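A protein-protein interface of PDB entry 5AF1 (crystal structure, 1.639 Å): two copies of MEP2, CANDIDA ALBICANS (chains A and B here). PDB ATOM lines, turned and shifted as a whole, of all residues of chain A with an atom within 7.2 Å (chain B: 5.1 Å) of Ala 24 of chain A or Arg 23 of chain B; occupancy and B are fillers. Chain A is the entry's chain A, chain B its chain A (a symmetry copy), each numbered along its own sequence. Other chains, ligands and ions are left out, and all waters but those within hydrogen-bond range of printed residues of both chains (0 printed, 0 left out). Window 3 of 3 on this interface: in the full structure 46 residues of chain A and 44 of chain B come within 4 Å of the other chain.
The side-chain carboxylate (OD1) of Asp 22 of chain A lies within hydrogen-bond range of the backbone NH (N) of Ala 24 of chain A, at 3.0 Å. The side-chain carboxylate (OD1) of Asp 22 of chain A lies within hydrogen-bond range of the backbone NH (N) of Asp 25 of chain A, at 3.0 Å. The side-chain hydroxyl (OG) of Ser 245 of chain A sits at hydrogen-bond distance from the side-chain carboxylate (OD1) of Asp 25 of chain A, at 2.7 Å. OD1 of Asn 244 of chain A lies within hydrogen-bond range of OG of Ser 246 of chain A (2.7 Å). The backbone carbonyl oxygen of Ser 246 of chain A sits at hydrogen-bond distance from the indole nitrogen of Trp 250 of chain A, at 3.3 Å. The backbone NH (N) of Ala 24 of chain B is in hydrogen-bond range of the side-chain carboxylate (OD1) of Asp 22 of chain B, 3.0 Å away.
Ala 24 of chain A touches Arg 23 of chain B, but with the chains exchanged Arg 23 of chain A does not touch Ala 24 of chain B (6.7 Å). Ala 24 of chain B touches its own counterpart, Ala 24 of chain A. Ala 24 of chain A touches Val 27 of chain B, but with the chains exchanged Val 27 of chain A does not touch Ala 24 of chain B (7.0 Å). Val 27 of chain B touches its own counterpart, Val 27 of chain A. Of the 16 pairs that touch across the chains among the printed residues, 2 have their exchanged pair printed and touching as well.
The side-chain carboxylate (OD1) of Asp 25 of chain A is in salt-bridge range of the guanidinium group (NH1) of Arg 23 of chain B, 3.7 Å away. OG of Ser 245 of chain A sits at hydrogen-bond distance from NH1 of Arg 23 of chain B. N of Met 247 of chain A is in hydrogen-bond range of OD1 of Asn 18 of chain B, at 2.8 Å. The side-chain sulfur of Met 26 of chain B sits close to the indole nitrogen of Trp 250 of chain A, 3.7 Å away. The side-chain amide nitrogen (ND2) of Asn 18 of chain B lies within hydrogen-bond range of the backbone carbonyl oxygen (O) of Ile 362 of chain A, at 3.0 Å. NH1 of Arg 23 of chain B lies close to N of Ser 246 of chain A (3.4 Å).
Ala 24 of chain A touches just these residues of chain B: Arg 23 (3.4 Å), Ala 24 (3.6 Å) and Val 27 (3.4 Å). Gly 30 of chain A touches none of the printed residues of chain B. Of the printed residues of chain B, Ser 245 of chain A touches Arg 23, Met 26 and Val 27. Printed residues of chain B within 4 Å of Ser 246 of chain A: Asn 18 and Arg 23. Of the printed residues of chain B, Ile 362 of chain A touches Asn 18 (3.0 Å). Of the printed residues of chain A, Phe 21 of chain B touches Met 247. Of chain A, only Ala 24 (3.4 Å), Asp 25 (3.7 Å), Ser 245 (3.0 Å) and Ser 246 (3.4 Å) come within 4 Å of Arg 23 of chain B. Of the printed residues of chain A, Val 27 of chain B touches Ala 24, Val 27, Trp 28, Ser 245 and Trp 250. The nearest printed residue of chain B that does not touch Ala 24 of chain A is Asp 25 of chain B (6.2 Å). The nearest printed residue of chain A that does not touch Asn 18 of chain B is Asp 363 of chain A (4.1 Å).
Of the 17 printed residues of chain A, 9 touch a printed residue of chain B. Hydrophobic or aromatic side chains of chain A within 4 Å of the printed part of chain B: Ala 24, Val 27, Trp 28, Met 247 and Trp 250. Printed residues of chain B that touch a printed residue of chain A: Asn 18, Phe 21, Arg 23, Ala 24, Met 26 and Val 27. Hydrophobic or aromatic side chains of chain B within 4 Å of the printed part of chain A: Phe 21, Met 26 and Val 27.
Among the printed residues, merely in contact across the chains: Ser 245 of chain A with Met 26 of chain B, Ala 24 of chain A with Arg 23 of chain B, Ala 24 of chain A with Val 27 of chain B, Ser 245 of chain A with Val 27 of chain B, Ser 246 of chain A with Asn 18 of chain B, Ala 24 of chain A with Ala 24 of chain B, Met 247 of chain A with Phe 21 of chain B, Trp 28 of chain A with Val 27 of chain B, Trp 250 of chain A with Val 27 of chain B and Val 27 of chain A with Val 27 of chain B.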
ATOM      1  N   PHE A  21      -4.312  -2.791  14.704  1.00  0.00           N
ATOM      2  CA  PHE A  21      -3.493  -1.708  14.161  1.00  0.00           C
ATOM      3  C   PHE A  21      -4.141  -0.358  14.402  1.00  0.00           C
ATOM      4  O   PHE A  21      -5.363  -0.241  14.445  1.00  0.00           O
ATOM      5  CB  PHE A  21      -3.251  -1.923  12.656  1.00  0.00           C
ATOM      6  CG  PHE A  21      -2.743  -3.302  12.330  1.00  0.00           C
ATOM      7  CD1 PHE A  21      -1.421  -3.641  12.576  1.00  0.00           C
ATOM      8  CD2 PHE A  21      -3.597  -4.271  11.821  1.00  0.00           C
ATOM      9  CE1 PHE A  21      -0.951  -4.929  12.314  1.00  0.00           C
ATOM     10  CE2 PHE A  21      -3.136  -5.561  11.551  1.00  0.00           C
ATOM     11  CZ  PHE A  21      -1.810  -5.889  11.799  1.00  0.00           C
ATOM     12  N   ASP A  22      -3.312   0.661  14.580  1.00  0.00           N
ATOM     13  CA  ASP A  22      -3.804   2.027  14.663  1.00  0.00           C
ATOM     14  C   ASP A  22      -4.170   2.461  13.243  1.00  0.00           C
ATOM     15  O   ASP A  22      -3.350   2.352  12.321  1.00  0.00           O
ATOM     16  CB  ASP A  22      -2.741   2.941  15.290  1.00  0.00           C
ATOM     17  CG  ASP A  22      -3.173   4.389  15.361  1.00  0.00           C
ATOM     18  OD1 ASP A  22      -3.017   5.099  14.355  1.00  0.00           O
ATOM     19  OD2 ASP A  22      -3.630   4.835  16.427  1.00  0.00           O
ATOM     20  N   ARG A  23      -5.409   2.911  13.055  1.00  0.00           N
ATOM     21  CA  ARG A  23      -5.859   3.263  11.699  1.00  0.00           C
ATOM     22  C   ARG A  23      -5.027   4.375  11.076  1.00  0.00           C
ATOM     23  O   ARG A  23      -4.763   4.344   9.874  1.00  0.00           O
ATOM     24  CB  ARG A  23      -7.332   3.682  11.703  1.00  0.00           C
ATOM     25  CG  ARG A  23      -8.312   2.606  12.170  1.00  0.00           C
ATOM     26  CD  ARG A  23      -8.191   1.335  11.351  1.00  0.00           C
ATOM     27  NE  ARG A  23      -9.303   0.413  11.617  1.00  0.00           N
ATOM     28  CZ  ARG A  23     -10.379   0.306  10.842  1.00  0.00           C
ATOM     29  NH1 ARG A  23     -10.485   1.060   9.756  1.00  0.00           N
ATOM     30  NH2 ARG A  23     -11.345  -0.552  11.150  1.00  0.00           N
ATOM     31  N   ALA A  24      -4.611   5.354  11.874  1.00  0.00           N
ATOM     32  CA  ALA A  24      -3.823   6.463  11.307  1.00  0.00           C
ATOM     33  C   ALA A  24      -2.434   5.996  10.863  1.00  0.00           C
ATOM     34  O   ALA A  24      -1.915   6.479   9.847  1.00  0.00           O
ATOM     35  CB  ALA A  24      -3.707   7.601  12.316  1.00  0.00           C
ATOM     36  N   ASP A  25      -1.836   5.061  11.609  1.00  0.00           N
ATOM     37  CA  ASP A  25      -0.587   4.408  11.162  1.00  0.00           C
ATOM     38  C   ASP A  25      -0.780   3.820   9.775  1.00  0.00           C
ATOM     39  O   ASP A  25       0.042   4.038   8.867  1.00  0.00           O
ATOM     40  CB  ASP A  25      -0.150   3.270  12.109  1.00  0.00           C
ATOM     41  CG  ASP A  25       0.398   3.757  13.443  1.00  0.00           C
ATOM     42  OD1 ASP A  25       0.599   4.972  13.639  1.00  0.00           O
ATOM     43  OD2 ASP A  25       0.635   2.886  14.313  1.00  0.00           O
ATOM     44  N   MET A  26      -1.874   3.082   9.594  1.00  0.00           N
ATOM     45  CA  MET A  26      -2.133   2.448   8.301  1.00  0.00           C
ATOM     46  C   MET A  26      -2.336   3.487   7.188  1.00  0.00           C
ATOM     47  O   MET A  26      -1.800   3.331   6.089  1.00  0.00           O
ATOM     48  CB  MET A  26      -3.349   1.520   8.378  1.00  0.00           C
ATOM     49  CG  MET A  26      -3.083   0.252   9.195  1.00  0.00           C
ATOM     50  SD  MET A  26      -4.238  -1.083   8.787  1.00  0.00           S
ATOM     51  CE  MET A  26      -5.717  -0.504   9.612  1.00  0.00           C
ATOM     52  N   VAL A  27      -3.113   4.535   7.467  1.00  0.00           N
ATOM     53  CA  VAL A  27      -3.351   5.561   6.440  1.00  0.00           C
ATOM     54  C   VAL A  27      -2.039   6.225   6.006  1.00  0.00           C
ATOM     55  O   VAL A  27      -1.816   6.434   4.805  1.00  0.00           O
ATOM     56  CB  VAL A  27      -4.345   6.644   6.926  1.00  0.00           C
ATOM     57  CG1 VAL A  27      -4.474   7.781   5.901  1.00  0.00           C
ATOM     58  CG2 VAL A  27      -5.715   6.032   7.165  1.00  0.00           C
ATOM     59  N   TRP A  28      -1.166   6.564   6.956  1.00  0.00           N
ATOM     60  CA  TRP A  28       0.096   7.195   6.543  1.00  0.00           C
ATOM     61  C   TRP A  28       0.941   6.241   5.689  1.00  0.00           C
ATOM     62  O   TRP A  28       1.511   6.654   4.682  1.00  0.00           O
ATOM     63  CB  TRP A  28       0.911   7.696   7.747  1.00  0.00           C
ATOM     64  CG  TRP A  28       2.287   8.204   7.336  1.00  0.00           C
ATOM     65  CD1 TRP A  28       3.488   7.776   7.813  1.00  0.00           C
ATOM     66  CD2 TRP A  28       2.583   9.202   6.334  1.00  0.00           C
ATOM     67  NE1 TRP A  28       4.518   8.451   7.181  1.00  0.00           N
ATOM     68  CE2 TRP A  28       3.987   9.334   6.280  1.00  0.00           C
ATOM     69  CE3 TRP A  28       1.796  10.006   5.507  1.00  0.00           C
ATOM     70  CZ2 TRP A  28       4.635  10.222   5.396  1.00  0.00           C
ATOM     71  CZ3 TRP A  28       2.441  10.899   4.618  1.00  0.00           C
ATOM     72  CH2 TRP A  28       3.844  10.992   4.584  1.00  0.00           C
ATOM     73  N   ILE A  29       1.007   4.962   6.047  1.00  0.00           N
ATOM     74  CA  ILE A  29       1.837   4.048   5.256  1.00  0.00           C
ATOM     75  C   ILE A  29       1.189   3.744   3.893  1.00  0.00           C
ATOM     76  O   ILE A  29       1.890   3.559   2.887  1.00  0.00           O
ATOM     77  CB  ILE A  29       2.140   2.753   6.053  1.00  0.00           C
ATOM     78  CG1 ILE A  29       2.859   3.115   7.360  1.00  0.00           C
ATOM     79  CG2 ILE A  29       2.984   1.778   5.219  1.00  0.00           C
ATOM     80  CD1 ILE A  29       4.060   4.067   7.174  1.00  0.00           C
ATOM     81  N   GLY A  30      -0.141   3.751   3.839  1.00  0.00           N
ATOM     82  CA  GLY A  30      -0.859   3.652   2.571  1.00  0.00           C
ATOM     83  C   GLY A  30      -0.537   4.842   1.676  1.00  0.00           C
ATOM     84  O   GLY A  30      -0.202   4.691   0.494  1.00  0.00           O
ATOM     85  N   ASN A 244       4.730   4.258  11.057  1.00  0.00           N
ATOM     86  CA  ASN A 244       3.666   4.781  11.919  1.00  0.00           C
ATOM     87  C   ASN A 244       3.365   6.262  11.680  1.00  0.00           C
ATOM     88  O   ASN A 244       4.007   6.925  10.850  1.00  0.00           O
ATOM     89  CB  ASN A 244       4.027   4.533  13.396  1.00  0.00           C
ATOM     90  CG  ASN A 244       5.265   5.299  13.828  1.00  0.00           C
ATOM     91  OD1 ASN A 244       5.409   6.482  13.519  1.00  0.00           O
ATOM     92  ND2 ASN A 244       6.168   4.626  14.547  1.00  0.00           N
ATOM     93  N   SER A 245       2.376   6.762  12.409  1.00  0.00           N
ATOM     94  CA  SER A 245       1.881   8.132  12.283  1.00  0.00           C
ATOM     95  C   SER A 245       2.497   9.063  13.324  1.00  0.00           C
ATOM     96  O   SER A 245       1.996  10.174  13.551  1.00  0.00           O
ATOM     97  CB  SER A 245       0.355   8.148  12.440  1.00  0.00           C
ATOM     98  OG  SER A 245      -0.023   7.563  13.684  1.00  0.00           O
ATOM     99  N   SER A 246       3.561   8.600  13.972  1.00  0.00           N
ATOM    100  CA  SER A 246       4.193   9.368  15.043  1.00  0.00           C
ATOM    101  C   SER A 246       4.916  10.579  14.482  1.00  0.00           C
ATOM    102  O   SER A 246       5.133  10.686  13.268  1.00  0.00           O
ATOM    103  CB  SER A 246       5.194   8.511  15.814  1.00  0.00           C
ATOM    104  OG  SER A 246       6.388   8.425  15.034  1.00  0.00           O
ATOM    105  N   MET A 247       5.345  11.470  15.369  1.00  0.00           N
ATOM    106  CA  MET A 247       6.057  12.640  14.889  1.00  0.00           C
ATOM    107  C   MET A 247       7.489  12.307  14.488  1.00  0.00           C
ATOM    108  O   MET A 247       8.171  13.159  13.935  1.00  0.00           O
ATOM    109  CB  MET A 247       6.029  13.766  15.917  1.00  0.00           C
ATOM    110  CG  MET A 247       6.818  13.496  17.177  1.00  0.00           C
ATOM    111  SD  MET A 247       6.649  14.837  18.390  1.00  0.00           S
ATOM    112  CE  MET A 247       5.057  14.418  19.110  1.00  0.00           C
ATOM    113  N   TRP A 250       7.368  12.830  10.816  1.00  0.00           N
ATOM    114  CA  TRP A 250       7.441  14.211  10.320  1.00  0.00           C
ATOM    115  C   TRP A 250       8.848  14.771  10.525  1.00  0.00           C
ATOM    116  O   TRP A 250       9.332  15.557   9.712  1.00  0.00           O
ATOM    117  CB  TRP A 250       6.369  15.085  11.008  1.00  0.00           C
ATOM    118  CG  TRP A 250       5.110  14.294  11.279  1.00  0.00           C
ATOM    119  CD1 TRP A 250       4.460  14.173  12.481  1.00  0.00           C
ATOM    120  CD2 TRP A 250       4.405  13.443  10.357  1.00  0.00           C
ATOM    121  NE1 TRP A 250       3.384  13.329  12.354  1.00  0.00           N
ATOM    122  CE2 TRP A 250       3.330  12.862  11.068  1.00  0.00           C
ATOM    123  CE3 TRP A 250       4.566  13.133   8.996  1.00  0.00           C
ATOM    124  CZ2 TRP A 250       2.423  11.986  10.468  1.00  0.00           C
ATOM    125  CZ3 TRP A 250       3.665  12.258   8.400  1.00  0.00           C
ATOM    126  CH2 TRP A 250       2.609  11.693   9.141  1.00  0.00           C
ATOM    127  N   ILE A 362      11.872   9.134  19.714  1.00  0.00           N
ATOM    128  CA  ILE A 362      10.712   9.992  19.484  1.00  0.00           C
ATOM    129  C   ILE A 362       9.409   9.188  19.329  1.00  0.00           C
ATOM    130  O   ILE A 362       8.336   9.644  19.724  1.00  0.00           O
ATOM    131  CB  ILE A 362      10.930  10.872  18.240  1.00  0.00           C
ATOM    132  CG1 ILE A 362      12.016  11.916  18.518  1.00  0.00           C
ATOM    133  CG2 ILE A 362       9.638  11.544  17.809  1.00  0.00           C
ATOM    134  CD1 ILE A 362      12.467  12.664  17.232  1.00  0.00           C
ATOM    135  N   ASP A 363       9.505   7.988  18.761  1.00  0.00           N
ATOM    136  CA  ASP A 363       8.346   7.105  18.692  1.00  0.00           C
ATOM    137  C   ASP A 363       8.592   5.817  19.469  1.00  0.00           C
ATOM    138  O   ASP A 363       7.961   4.795  19.204  1.00  0.00           O
ATOM    139  CB  ASP A 363       7.976   6.777  17.238  1.00  0.00           C
ATOM    140  CG  ASP A 363       9.057   5.990  16.509  1.00  0.00           C
ATOM    141  OD1 ASP A 363      10.087   5.639  17.128  1.00  0.00           O
ATOM    142  OD2 ASP A 363       8.869   5.712  15.296  1.00  0.00           O
ATOM    143  N   ASP B  16       5.754   9.721  26.113  1.00  0.00           N
ATOM    144  CA  ASP B  16       5.479   9.596  24.687  1.00  0.00           C
ATOM    145  C   ASP B  16       4.825  10.893  24.225  1.00  0.00           C
ATOM    146  O   ASP B  16       3.646  11.126  24.488  1.00  0.00           O
ATOM    147  CB  ASP B  16       4.576   8.381  24.428  1.00  0.00           C
ATOM    148  CG  ASP B  16       4.179   8.230  22.970  1.00  0.00           C
ATOM    149  OD1 ASP B  16       4.712   8.963  22.117  1.00  0.00           O
ATOM    150  OD2 ASP B  16       3.329   7.356  22.691  1.00  0.00           O
ATOM    151  N   ASN B  18       3.798  11.819  21.510  1.00  0.00           N
ATOM    152  CA  ASN B  18       2.719  11.633  20.543  1.00  0.00           C
ATOM    153  C   ASN B  18       1.338  11.525  21.193  1.00  0.00           C
ATOM    154  O   ASN B  18       0.321  11.725  20.520  1.00  0.00           O
ATOM    155  CB  ASN B  18       2.990  10.391  19.695  1.00  0.00           C
ATOM    156  CG  ASN B  18       4.292  10.493  18.947  1.00  0.00           C
ATOM    157  OD1 ASN B  18       4.392  11.240  17.978  1.00  0.00           O
ATOM    158  ND2 ASN B  18       5.311   9.773  19.417  1.00  0.00           N
ATOM    159  N   PHE B  21      -1.464  14.310  20.808  1.00  0.00           N
ATOM    160  CA  PHE B  21      -2.030  14.656  19.506  1.00  0.00           C
ATOM    161  C   PHE B  21      -2.859  13.514  18.949  1.00  0.00           C
ATOM    162  O   PHE B  21      -2.583  12.346  19.208  1.00  0.00           O
ATOM    163  CB  PHE B  21      -0.910  15.033  18.519  1.00  0.00           C
ATOM    164  CG  PHE B  21       0.041  16.062  19.069  1.00  0.00           C
ATOM    165  CD1 PHE B  21      -0.328  17.396  19.136  1.00  0.00           C
ATOM    166  CD2 PHE B  21       1.285  15.688  19.559  1.00  0.00           C
ATOM    167  CE1 PHE B  21       0.532  18.351  19.682  1.00  0.00           C
ATOM    168  CE2 PHE B  21       2.155  16.635  20.102  1.00  0.00           C
ATOM    169  CZ  PHE B  21       1.776  17.968  20.163  1.00  0.00           C
ATOM    170  N   ASP B  22      -3.894  13.862  18.198  1.00  0.00           N
ATOM    171  CA  ASP B  22      -4.673  12.864  17.479  1.00  0.00           C
ATOM    172  C   ASP B  22      -3.837  12.422  16.277  1.00  0.00           C
ATOM    173  O   ASP B  22      -3.375  13.259  15.489  1.00  0.00           O
ATOM    174  CB  ASP B  22      -6.029  13.446  17.057  1.00  0.00           C
ATOM    175  CG  ASP B  22      -6.869  12.471  16.260  1.00  0.00           C
ATOM    176  OD1 ASP B  22      -6.665  12.379  15.040  1.00  0.00           O
ATOM    177  OD2 ASP B  22      -7.761  11.826  16.838  1.00  0.00           O
ATOM    178  N   ARG B  23      -3.605  11.116  16.156  1.00  0.00           N
ATOM    179  CA  ARG B  23      -2.735  10.626  15.074  1.00  0.00           C
ATOM    180  C   ARG B  23      -3.268  10.975  13.692  1.00  0.00           C
ATOM    181  O   ARG B  23      -2.486  11.286  12.794  1.00  0.00           O
ATOM    182  CB  ARG B  23      -2.547   9.110  15.169  1.00  0.00           C
ATOM    183  CG  ARG B  23      -1.881   8.617  16.454  1.00  0.00           C
ATOM    184  CD  ARG B  23      -0.532   9.271  16.680  1.00  0.00           C
ATOM    185  NE  ARG B  23       0.219   8.606  17.754  1.00  0.00           N
ATOM    186  CZ  ARG B  23       1.168   7.699  17.543  1.00  0.00           C
ATOM    187  NH1 ARG B  23       1.482   7.352  16.302  1.00  0.00           N
ATOM    188  NH2 ARG B  23       1.802   7.140  18.567  1.00  0.00           N
ATOM    189  N   ALA B  24      -4.585  10.932  13.510  1.00  0.00           N
ATOM    190  CA  ALA B  24      -5.142  11.239  12.179  1.00  0.00           C
ATOM    191  C   ALA B  24      -4.964  12.719  11.825  1.00  0.00           C
ATOM    192  O   ALA B  24      -4.721  13.049  10.657  1.00  0.00           O
ATOM    193  CB  ALA B  24      -6.615  10.848  12.117  1.00  0.00           C
ATOM    194  N   ASP B  25      -5.078  13.604  12.821  1.00  0.00           N
ATOM    195  CA  ASP B  25      -4.737  15.028  12.622  1.00  0.00           C
ATOM    196  C   ASP B  25      -3.326  15.149  12.074  1.00  0.00           C
ATOM    197  O   ASP B  25      -3.085  15.858  11.080  1.00  0.00           O
ATOM    198  CB  ASP B  25      -4.813  15.838  13.935  1.00  0.00           C
ATOM    199  CG  ASP B  25      -6.233  16.084  14.425  1.00  0.00           C
ATOM    200  OD1 ASP B  25      -7.210  15.776  13.713  1.00  0.00           O
ATOM    201  OD2 ASP B  25      -6.362  16.607  15.556  1.00  0.00           O
ATOM    202  N   MET B  26      -2.386  14.449  12.705  1.00  0.00           N
ATOM    203  CA  MET B  26      -0.991  14.522  12.269  1.00  0.00           C
ATOM    204  C   MET B  26      -0.808  13.975  10.846  1.00  0.00           C
ATOM    205  O   MET B  26      -0.103  14.579  10.035  1.00  0.00           O
ATOM    206  CB  MET B  26      -0.072  13.773  13.238  1.00  0.00           C
ATOM    207  CG  MET B  26       0.080  14.482  14.587  1.00  0.00           C
ATOM    208  SD  MET B  26       1.581  13.973  15.465  1.00  0.00           S
ATOM    209  CE  MET B  26       1.093  12.350  16.040  1.00  0.00           C
ATOM    210  N   VAL B  27      -1.432  12.833  10.547  1.00  0.00           N
ATOM    211  CA  VAL B  27      -1.291  12.255   9.201  1.00  0.00           C
ATOM    212  C   VAL B  27      -1.820  13.214   8.129  1.00  0.00           C
ATOM    213  O   VAL B  27      -1.179  13.392   7.082  1.00  0.00           O
ATOM    214  CB  VAL B  27      -2.015  10.892   9.082  1.00  0.00           C
ATOM    215  CG1 VAL B  27      -1.980  10.369   7.637  1.00  0.00           C
ATOM    216  CG2 VAL B  27      -1.363   9.868   9.996  1.00  0.00           C
